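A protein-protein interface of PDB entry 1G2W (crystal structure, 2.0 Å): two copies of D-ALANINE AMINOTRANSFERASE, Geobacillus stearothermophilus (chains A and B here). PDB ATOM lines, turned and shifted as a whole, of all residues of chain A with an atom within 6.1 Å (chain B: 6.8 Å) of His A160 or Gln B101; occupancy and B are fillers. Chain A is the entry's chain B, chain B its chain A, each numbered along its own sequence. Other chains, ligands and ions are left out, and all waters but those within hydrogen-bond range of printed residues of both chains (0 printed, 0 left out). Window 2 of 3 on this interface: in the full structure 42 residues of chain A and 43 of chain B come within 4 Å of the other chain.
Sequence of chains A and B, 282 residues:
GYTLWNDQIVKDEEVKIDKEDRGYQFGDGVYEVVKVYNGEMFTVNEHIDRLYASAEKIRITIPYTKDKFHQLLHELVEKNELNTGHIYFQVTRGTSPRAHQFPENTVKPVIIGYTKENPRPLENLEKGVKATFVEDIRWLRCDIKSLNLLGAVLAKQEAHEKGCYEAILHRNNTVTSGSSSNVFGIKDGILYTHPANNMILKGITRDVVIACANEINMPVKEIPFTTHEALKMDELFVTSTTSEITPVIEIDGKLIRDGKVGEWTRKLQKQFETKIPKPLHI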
ATOM      1  N   ALA A 152      16.931 -17.243   4.174  1.00  0.00           N
ATOM      2  CA  ALA A 152      17.102 -17.563   5.587  1.00  0.00           C
ATOM      3  C   ALA A 152      17.211 -19.070   5.771  1.00  0.00           C
ATOM      4  O   ALA A 152      18.001 -19.554   6.585  1.00  0.00           O
ATOM      5  CB  ALA A 152      15.922 -17.017   6.390  1.00  0.00           C
ATOM      6  N   VAL A 153      16.406 -19.812   5.016  1.00  0.00           N
ATOM      7  CA  VAL A 153      16.424 -21.266   5.089  1.00  0.00           C
ATOM      8  C   VAL A 153      17.796 -21.823   4.723  1.00  0.00           C
ATOM      9  O   VAL A 153      18.335 -22.673   5.434  1.00  0.00           O
ATOM     10  CB  VAL A 153      15.371 -21.894   4.157  1.00  0.00           C
ATOM     11  CG1 VAL A 153      15.660 -23.382   3.960  1.00  0.00           C
ATOM     12  CG2 VAL A 153      13.981 -21.707   4.756  1.00  0.00           C
ATOM     13  N   ALA A 155      20.636 -20.217   4.749  1.00  0.00           N
ATOM     14  CA  ALA A 155      21.633 -19.727   5.704  1.00  0.00           C
ATOM     15  C   ALA A 155      21.602 -20.535   6.998  1.00  0.00           C
ATOM     16  O   ALA A 155      22.646 -20.969   7.494  1.00  0.00           O
ATOM     17  CB  ALA A 155      21.387 -18.266   6.007  1.00  0.00           C
ATOM     18  N   LYS A 156      20.406 -20.735   7.545  1.00  0.00           N
ATOM     19  CA  LYS A 156      20.268 -21.502   8.780  1.00  0.00           C
ATOM     20  C   LYS A 156      20.764 -22.943   8.609  1.00  0.00           C
ATOM     21  O   LYS A 156      21.418 -23.490   9.497  1.00  0.00           O
ATOM     22  CB  LYS A 156      18.811 -21.529   9.240  1.00  0.00           C
ATOM     23  CG  LYS A 156      18.617 -22.213  10.585  1.00  0.00           C
ATOM     24  CD  LYS A 156      19.033 -21.305  11.734  1.00  0.00           C
ATOM     25  CE  LYS A 156      18.087 -20.112  11.833  1.00  0.00           C
ATOM     26  NZ  LYS A 156      18.416 -19.203  12.970  1.00  0.00           N
ATOM     27  N   GLN A 157      20.446 -23.556   7.474  1.00  0.00           N
ATOM     28  CA  GLN A 157      20.867 -24.926   7.220  1.00  0.00           C
ATOM     29  C   GLN A 157      22.388 -25.033   7.181  1.00  0.00           C
ATOM     30  O   GLN A 157      22.962 -25.995   7.698  1.00  0.00           O
ATOM     31  CB  GLN A 157      20.270 -25.430   5.905  1.00  0.00           C
ATOM     32  CG  GLN A 157      20.618 -26.874   5.564  1.00  0.00           C
ATOM     33  CD  GLN A 157      20.302 -27.839   6.698  1.00  0.00           C
ATOM     34  OE1 GLN A 157      19.317 -27.671   7.420  1.00  0.00           O
ATOM     35  NE2 GLN A 157      21.130 -28.868   6.846  1.00  0.00           N
ATOM     36  N   GLU A 158      23.040 -24.050   6.566  1.00  0.00           N
ATOM     37  CA  GLU A 158      24.496 -24.051   6.493  1.00  0.00           C
ATOM     38  C   GLU A 158      25.033 -23.986   7.919  1.00  0.00           C
ATOM     39  O   GLU A 158      25.953 -24.708   8.283  1.00  0.00           O
ATOM     40  CB  GLU A 158      25.006 -22.843   5.696  1.00  0.00           C
ATOM     41  CG  GLU A 158      26.497 -22.898   5.407  1.00  0.00           C
ATOM     42  CD  GLU A 158      26.977 -21.773   4.491  1.00  0.00           C
ATOM     43  OE1 GLU A 158      26.295 -21.476   3.488  1.00  0.00           O
ATOM     44  OE2 GLU A 158      28.047 -21.196   4.774  1.00  0.00           O
ATOM     45  N   ALA A 159      24.441 -23.114   8.725  1.00  0.00           N
ATOM     46  CA  ALA A 159      24.855 -22.961  10.115  1.00  0.00           C
ATOM     47  C   ALA A 159      24.655 -24.266  10.896  1.00  0.00           C
ATOM     48  O   ALA A 159      25.562 -24.725  11.593  1.00  0.00           O
ATOM     49  CB  ALA A 159      24.064 -21.830  10.767  1.00  0.00           C
ATOM     50  N   HIS A 160      23.472 -24.863  10.770  1.00  0.00           N
ATOM     51  CA  HIS A 160      23.163 -26.105  11.469  1.00  0.00           C
ATOM     52  C   HIS A 160      24.154 -27.201  11.068  1.00  0.00           C
ATOM     53  O   HIS A 160      24.672 -27.918  11.926  1.00  0.00           O
ATOM     54  CB  HIS A 160      21.724 -26.533  11.163  1.00  0.00           C
ATOM     55  CG  HIS A 160      21.203 -27.607  12.067  1.00  0.00           C
ATOM     56  ND1 HIS A 160      21.621 -28.920  11.987  1.00  0.00           N
ATOM     57  CD2 HIS A 160      20.296 -27.564  13.071  1.00  0.00           C
ATOM     58  CE1 HIS A 160      20.993 -29.637  12.901  1.00  0.00           C
ATOM     59  NE2 HIS A 160      20.183 -28.837  13.574  1.00  0.00           N
ATOM     60  N   GLU A 161      24.431 -27.321   9.773  1.00  0.00           N
ATOM     61  CA  GLU A 161      25.373 -28.329   9.290  1.00  0.00           C
ATOM     62  C   GLU A 161      26.757 -28.193   9.922  1.00  0.00           C
ATOM     63  O   GLU A 161      27.488 -29.177  10.039  1.00  0.00           O
ATOM     64  CB  GLU A 161      25.500 -28.251   7.766  1.00  0.00           C
ATOM     65  CG  GLU A 161      24.544 -29.167   7.021  1.00  0.00           C
ATOM     66  CD  GLU A 161      24.480 -28.868   5.537  1.00  0.00           C
ATOM     67  OE1 GLU A 161      25.541 -28.593   4.930  1.00  0.00           O
ATOM     68  OE2 GLU A 161      23.365 -28.915   4.976  1.00  0.00           O
ATOM     69  N   LYS A 162      27.114 -26.976  10.323  1.00  0.00           N
ATOM     70  CA  LYS A 162      28.412 -26.718  10.945  1.00  0.00           C
ATOM     71  C   LYS A 162      28.325 -26.771  12.467  1.00  0.00           C
ATOM     72  O   LYS A 162      29.295 -26.462  13.158  1.00  0.00           O
ATOM     73  CB  LYS A 162      28.943 -25.346  10.527  1.00  0.00           C
ATOM     74  CG  LYS A 162      29.325 -25.212   9.061  1.00  0.00           C
ATOM     75  CD  LYS A 162      29.684 -23.764   8.756  1.00  0.00           C
ATOM     76  CE  LYS A 162      30.119 -23.558   7.320  1.00  0.00           C
ATOM     77  NZ  LYS A 162      30.284 -22.104   7.023  1.00  0.00           N
ATOM     78  N   GLY A 163      27.161 -27.149  12.988  1.00  0.00           N
ATOM     79  CA  GLY A 163      26.995 -27.228  14.427  1.00  0.00           C
ATOM     80  C   GLY A 163      26.885 -25.858  15.068  1.00  0.00           C
ATOM     81  O   GLY A 163      27.223 -25.677  16.237  1.00  0.00           O
ATOM     82  N   CYS A 164      26.411 -24.883  14.299  1.00  0.00           N
ATOM     83  CA  CYS A 164      26.249 -23.529  14.803  1.00  0.00           C
ATOM     84  C   CYS A 164      24.785 -23.228  14.990  1.00  0.00           C
ATOM     85  O   CYS A 164      23.932 -23.790  14.310  1.00  0.00           O
ATOM     86  CB  CYS A 164      26.844 -22.512  13.836  1.00  0.00           C
ATOM     87  SG  CYS A 164      28.599 -22.696  13.630  1.00  0.00           S
ATOM     88  N   TYR A 165      24.500 -22.319  15.908  1.00  0.00           N
ATOM     89  CA  TYR A 165      23.134 -21.942  16.197  1.00  0.00           C
ATOM     90  C   TYR A 165      22.542 -21.010  15.148  1.00  0.00           C
ATOM     91  O   TYR A 165      21.414 -21.210  14.688  1.00  0.00           O
ATOM     92  CB  TYR A 165      23.074 -21.259  17.557  1.00  0.00           C
ATOM     93  CG  TYR A 165      21.693 -20.788  17.934  1.00  0.00           C
ATOM     94  CD1 TYR A 165      20.694 -21.702  18.283  1.00  0.00           C
ATOM     95  CD2 TYR A 165      21.381 -19.430  17.940  1.00  0.00           C
ATOM     96  CE1 TYR A 165      19.421 -21.265  18.636  1.00  0.00           C
ATOM     97  CE2 TYR A 165      20.118 -18.987  18.288  1.00  0.00           C
ATOM     98  CZ  TYR A 165      19.145 -19.907  18.635  1.00  0.00           C
ATOM     99  OH  TYR A 165      17.905 -19.458  19.002  1.00  0.00           O
ATOM    100  N   ARG B  22       6.227 -26.428   3.802  1.00  0.00           N
ATOM    101  CA  ARG B  22       7.280 -25.414   3.755  1.00  0.00           C
ATOM    102  C   ARG B  22       7.167 -24.465   2.561  1.00  0.00           C
ATOM    103  O   ARG B  22       7.784 -23.398   2.544  1.00  0.00           O
ATOM    104  CB  ARG B  22       8.659 -26.072   3.787  1.00  0.00           C
ATOM    105  CG  ARG B  22       9.004 -26.694   5.138  1.00  0.00           C
ATOM    106  CD  ARG B  22      10.296 -27.489   5.048  1.00  0.00           C
ATOM    107  NE  ARG B  22      11.454 -26.625   4.815  1.00  0.00           N
ATOM    108  CZ  ARG B  22      12.158 -26.049   5.785  1.00  0.00           C
ATOM    109  NH1 ARG B  22      11.822 -26.252   7.050  1.00  0.00           N
ATOM    110  NH2 ARG B  22      13.189 -25.269   5.493  1.00  0.00           N
ATOM    111  N   PHE B  26       7.668 -20.719   3.815  1.00  0.00           N
ATOM    112  CA  PHE B  26       8.965 -20.174   3.425  1.00  0.00           C
ATOM    113  C   PHE B  26       9.129 -19.944   1.922  1.00  0.00           C
ATOM    114  O   PHE B  26      10.110 -19.328   1.492  1.00  0.00           O
ATOM    115  CB  PHE B  26      10.090 -21.124   3.871  1.00  0.00           C
ATOM    116  CG  PHE B  26      10.113 -21.401   5.350  1.00  0.00           C
ATOM    117  CD1 PHE B  26      10.395 -20.389   6.261  1.00  0.00           C
ATOM    118  CD2 PHE B  26       9.856 -22.682   5.830  1.00  0.00           C
ATOM    119  CE1 PHE B  26      10.420 -20.648   7.629  1.00  0.00           C
ATOM    120  CE2 PHE B  26       9.878 -22.954   7.199  1.00  0.00           C
ATOM    121  CZ  PHE B  26      10.161 -21.932   8.101  1.00  0.00           C
ATOM    122  N   ASP B  28       9.598 -22.296   0.170  1.00  0.00           N
ATOM    123  CA  ASP B  28      10.661 -23.287   0.025  1.00  0.00           C
ATOM    124  C   ASP B  28      10.329 -24.356  -1.011  1.00  0.00           C
ATOM    125  O   ASP B  28       9.956 -25.490  -0.672  1.00  0.00           O
ATOM    126  CB  ASP B  28      10.938 -23.927   1.391  1.00  0.00           C
ATOM    127  CG  ASP B  28      12.179 -24.796   1.395  1.00  0.00           C
ATOM    128  OD1 ASP B  28      12.934 -24.786   0.395  1.00  0.00           O
ATOM    129  OD2 ASP B  28      12.405 -25.482   2.413  1.00  0.00           O
ATOM    130  N   ARG B  93       9.680 -28.524  -0.278  1.00  0.00           N
ATOM    131  CA  ARG B  93      10.428 -29.452   0.555  1.00  0.00           C
ATOM    132  C   ARG B  93       9.527 -30.391   1.377  1.00  0.00           C
ATOM    133  O   ARG B  93       9.980 -31.435   1.848  1.00  0.00           O
ATOM    134  CB  ARG B  93      11.385 -28.681   1.476  1.00  0.00           C
ATOM    135  CG  ARG B  93      12.536 -29.524   2.003  1.00  0.00           C
ATOM    136  CD  ARG B  93      13.479 -28.685   2.859  1.00  0.00           C
ATOM    137  NE  ARG B  93      13.958 -27.520   2.122  1.00  0.00           N
ATOM    138  CZ  ARG B  93      14.968 -27.537   1.260  1.00  0.00           C
ATOM    139  NH1 ARG B  93      15.632 -28.660   1.021  1.00  0.00           N
ATOM    140  NH2 ARG B  93      15.299 -26.427   0.617  1.00  0.00           N
ATOM    141  N   SER B  96       6.425 -30.049   7.587  1.00  0.00           N
ATOM    142  CA  SER B  96       7.191 -30.326   8.785  1.00  0.00           C
ATOM    143  C   SER B  96       6.973 -29.186   9.776  1.00  0.00           C
ATOM    144  O   SER B  96       6.712 -28.051   9.372  1.00  0.00           O
ATOM    145  CB  SER B  96       8.671 -30.428   8.403  1.00  0.00           C
ATOM    146  OG  SER B  96       9.486 -30.664   9.530  1.00  0.00           O
ATOM    147  N   PRO B  97       7.059 -29.473  11.088  1.00  0.00           N
ATOM    148  CA  PRO B  97       6.864 -28.409  12.082  1.00  0.00           C
ATOM    149  C   PRO B  97       7.759 -27.236  11.699  1.00  0.00           C
ATOM    150  O   PRO B  97       8.934 -27.429  11.399  1.00  0.00           O
ATOM    151  CB  PRO B  97       7.295 -29.075  13.387  1.00  0.00           C
ATOM    152  CG  PRO B  97       6.899 -30.518  13.163  1.00  0.00           C
ATOM    153  CD  PRO B  97       7.350 -30.766  11.739  1.00  0.00           C
ATOM    154  N   ARG B  98       7.205 -26.029  11.706  1.00  0.00           N
ATOM    155  CA  ARG B  98       7.956 -24.846  11.310  1.00  0.00           C
ATOM    156  C   ARG B  98       9.342 -24.653  11.918  1.00  0.00           C
ATOM    157  O   ARG B  98       9.500 -24.473  13.130  1.00  0.00           O
ATOM    158  CB  ARG B  98       7.135 -23.580  11.548  1.00  0.00           C
ATOM    159  CG  ARG B  98       7.838 -22.328  11.031  1.00  0.00           C
ATOM    160  CD  ARG B  98       6.931 -21.120  11.059  1.00  0.00           C
ATOM    161  NE  ARG B  98       7.523 -19.971  10.379  1.00  0.00           N
ATOM    162  CZ  ARG B  98       8.490 -19.211  10.882  1.00  0.00           C
ATOM    163  NH1 ARG B  98       8.986 -19.469  12.086  1.00  0.00           N
ATOM    164  NH2 ARG B  98       8.961 -18.186  10.177  1.00  0.00           N
ATOM    165  N   ALA B  99      10.341 -24.672  11.041  1.00  0.00           N
ATOM    166  CA  ALA B  99      11.737 -24.471  11.409  1.00  0.00           C
ATOM    167  C   ALA B  99      12.482 -24.079  10.128  1.00  0.00           C
ATOM    168  O   ALA B  99      12.215 -24.639   9.068  1.00  0.00           O
ATOM    169  CB  ALA B  99      12.311 -25.753  11.982  1.00  0.00           C
ATOM    170  N   HIS B 100      13.409 -23.126  10.216  1.00  0.00           N
ATOM    171  CA  HIS B 100      14.157 -22.696   9.031  1.00  0.00           C
ATOM    172  C   HIS B 100      15.039 -23.780   8.430  1.00  0.00           C
ATOM    173  O   HIS B 100      15.043 -23.968   7.214  1.00  0.00           O
ATOM    174  CB  HIS B 100      15.027 -21.477   9.337  1.00  0.00           C
ATOM    175  CG  HIS B 100      14.245 -20.238   9.620  1.00  0.00           C
ATOM    176  ND1 HIS B 100      13.519 -20.064  10.777  1.00  0.00           N
ATOM    177  CD2 HIS B 100      14.052 -19.119   8.882  1.00  0.00           C
ATOM    178  CE1 HIS B 100      12.913 -18.893  10.741  1.00  0.00           C
ATOM    179  NE2 HIS B 100      13.220 -18.299   9.602  1.00  0.00           N
ATOM    180  N   GLN B 101      15.800 -24.480   9.268  1.00  0.00           N
ATOM    181  CA  GLN B 101      16.674 -25.541   8.769  1.00  0.00           C
ATOM    182  C   GLN B 101      15.865 -26.676   8.144  1.00  0.00           C
ATOM    183  O   GLN B 101      14.651 -26.769   8.336  1.00  0.00           O
ATOM    184  CB  GLN B 101      17.585 -26.092   9.879  1.00  0.00           C
ATOM    185  CG  GLN B 101      16.903 -26.518  11.170  1.00  0.00           C
ATOM    186  CD  GLN B 101      16.469 -25.335  12.012  1.00  0.00           C
ATOM    187  OE1 GLN B 101      15.377 -24.800  11.838  1.00  0.00           O
ATOM    188  NE2 GLN B 101      17.336 -24.908  12.919  1.00  0.00           N
ATOM    189  N   PHE B 102      16.542 -27.534   7.386  1.00  0.00           N
ATOM    190  CA  PHE B 102      15.882 -28.652   6.722  1.00  0.00           C
ATOM    191  C   PHE B 102      15.346 -29.690   7.711  1.00  0.00           C
ATOM    192  O   PHE B 102      15.914 -29.888   8.787  1.00  0.00           O
ATOM    193  CB  PHE B 102      16.850 -29.382   5.779  1.00  0.00           C
ATOM    194  CG  PHE B 102      17.422 -28.529   4.676  1.00  0.00           C
ATOM    195  CD1 PHE B 102      16.895 -27.276   4.375  1.00  0.00           C
ATOM    196  CD2 PHE B 102      18.489 -29.008   3.918  1.00  0.00           C
ATOM    197  CE1 PHE B 102      17.431 -26.505   3.331  1.00  0.00           C
ATOM    198  CE2 PHE B 102      19.029 -28.251   2.879  1.00  0.00           C
ATOM    199  CZ  PHE B 102      18.499 -26.998   2.584  1.00  0.00           C
ATOM    200  N   PRO B 103      14.243 -30.362   7.351  1.00  0.00           N
ATOM    201  CA  PRO B 103      13.641 -31.394   8.199  1.00  0.00           C
ATOM    202  C   PRO B 103      14.523 -32.625   7.981  1.00  0.00           C
ATOM    203  O   PRO B 103      15.279 -32.656   7.010  1.00  0.00           O
ATOM    204  CB  PRO B 103      12.255 -31.585   7.584  1.00  0.00           C
ATOM    205  CG  PRO B 103      12.007 -30.295   6.845  1.00  0.00           C
ATOM    206  CD  PRO B 103      13.338 -30.006   6.247  1.00  0.00           C
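Among the printed residues, no Asp or Glu carboxylate lies within 4 Å of a Lys or Arg side-chain nitrogen of the other chain.
No position is printed for both chains. Of the 10 pairs that touch across the chains among the printed residues, none has its exchanged pair printed and touching as well.
The guanidinium group of Arg B22 lies within hydrogen-bond range of the backbone carbonyl oxygen of His B100 (2.8 Å). The guanidinium group (NH1) of Arg B22 sits at hydrogen-bond distance from the backbone carbonyl oxygen (O) of Ala B99 (2.6 Å). The backbone carbonyl oxygen (O) of Gln B101 is in hydrogen-bond range of the guanidinium group (NH1) of Arg B22 (3.2 Å). The guanidinium group (NE) of Arg B22 is in salt-bridge range of the side-chain carboxylate (OD2) of Asp B28 (2.8 Å). OE2 of Glu A161 is in hydrogen-bond range of NE2 of Gln A157, 2.9 Å away.
His A160 touches just one residue of chain B: Gln B101. Gln B101 touches just these residues of chain A: Lys A156, Gln A157 and His A160. Of the printed residues of chain B, Lys A156 touches His B100 (3.8 Å) and Gln B101 (3.8 Å). Printed residues of chain B within 4 Å of Val A153: Arg B22 (3.5 Å), Phe B26 (3.9 Å), His B100 (3.4 Å) and Phe B102 (3.6 Å). Of the printed residues of chain A, His B100 touches Ala A152, Val A153 and Lys A156. Printed residues of chain A within 4 Å of Arg B22: Val A153 (3.5 Å). Glu A161 touches none of the printed residues of chain B. The nearest residue of chain B that does not touch His A160 is Phe B102 (6.5 Å). The nearest printed residue of chain B that does not touch Val A153 is Asp B28 (4.2 Å).
Among the printed residues, merely in contact across the chains: Ala A152 with His B100 (3.8 Å), Val A153 with Arg B22 (3.5 Å), Val A153 with Phe B26 (3.9 Å), Val A153 with His B100 (3.4 Å), Val A153 with Phe B102 (3.6 Å), Lys A156 with His B100 (3.8 Å), Lys A156 with Gln B101 (3.8 Å), Gln A157 with Gln B101 (3.4 Å) and His A160 with Gln B101 (3.98 Å).
The side-chain amide oxygen (OE1) of Gln A157 is in hydrogen-bond range of the backbone NH (N) of Phe B102, 2.8 Å away.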
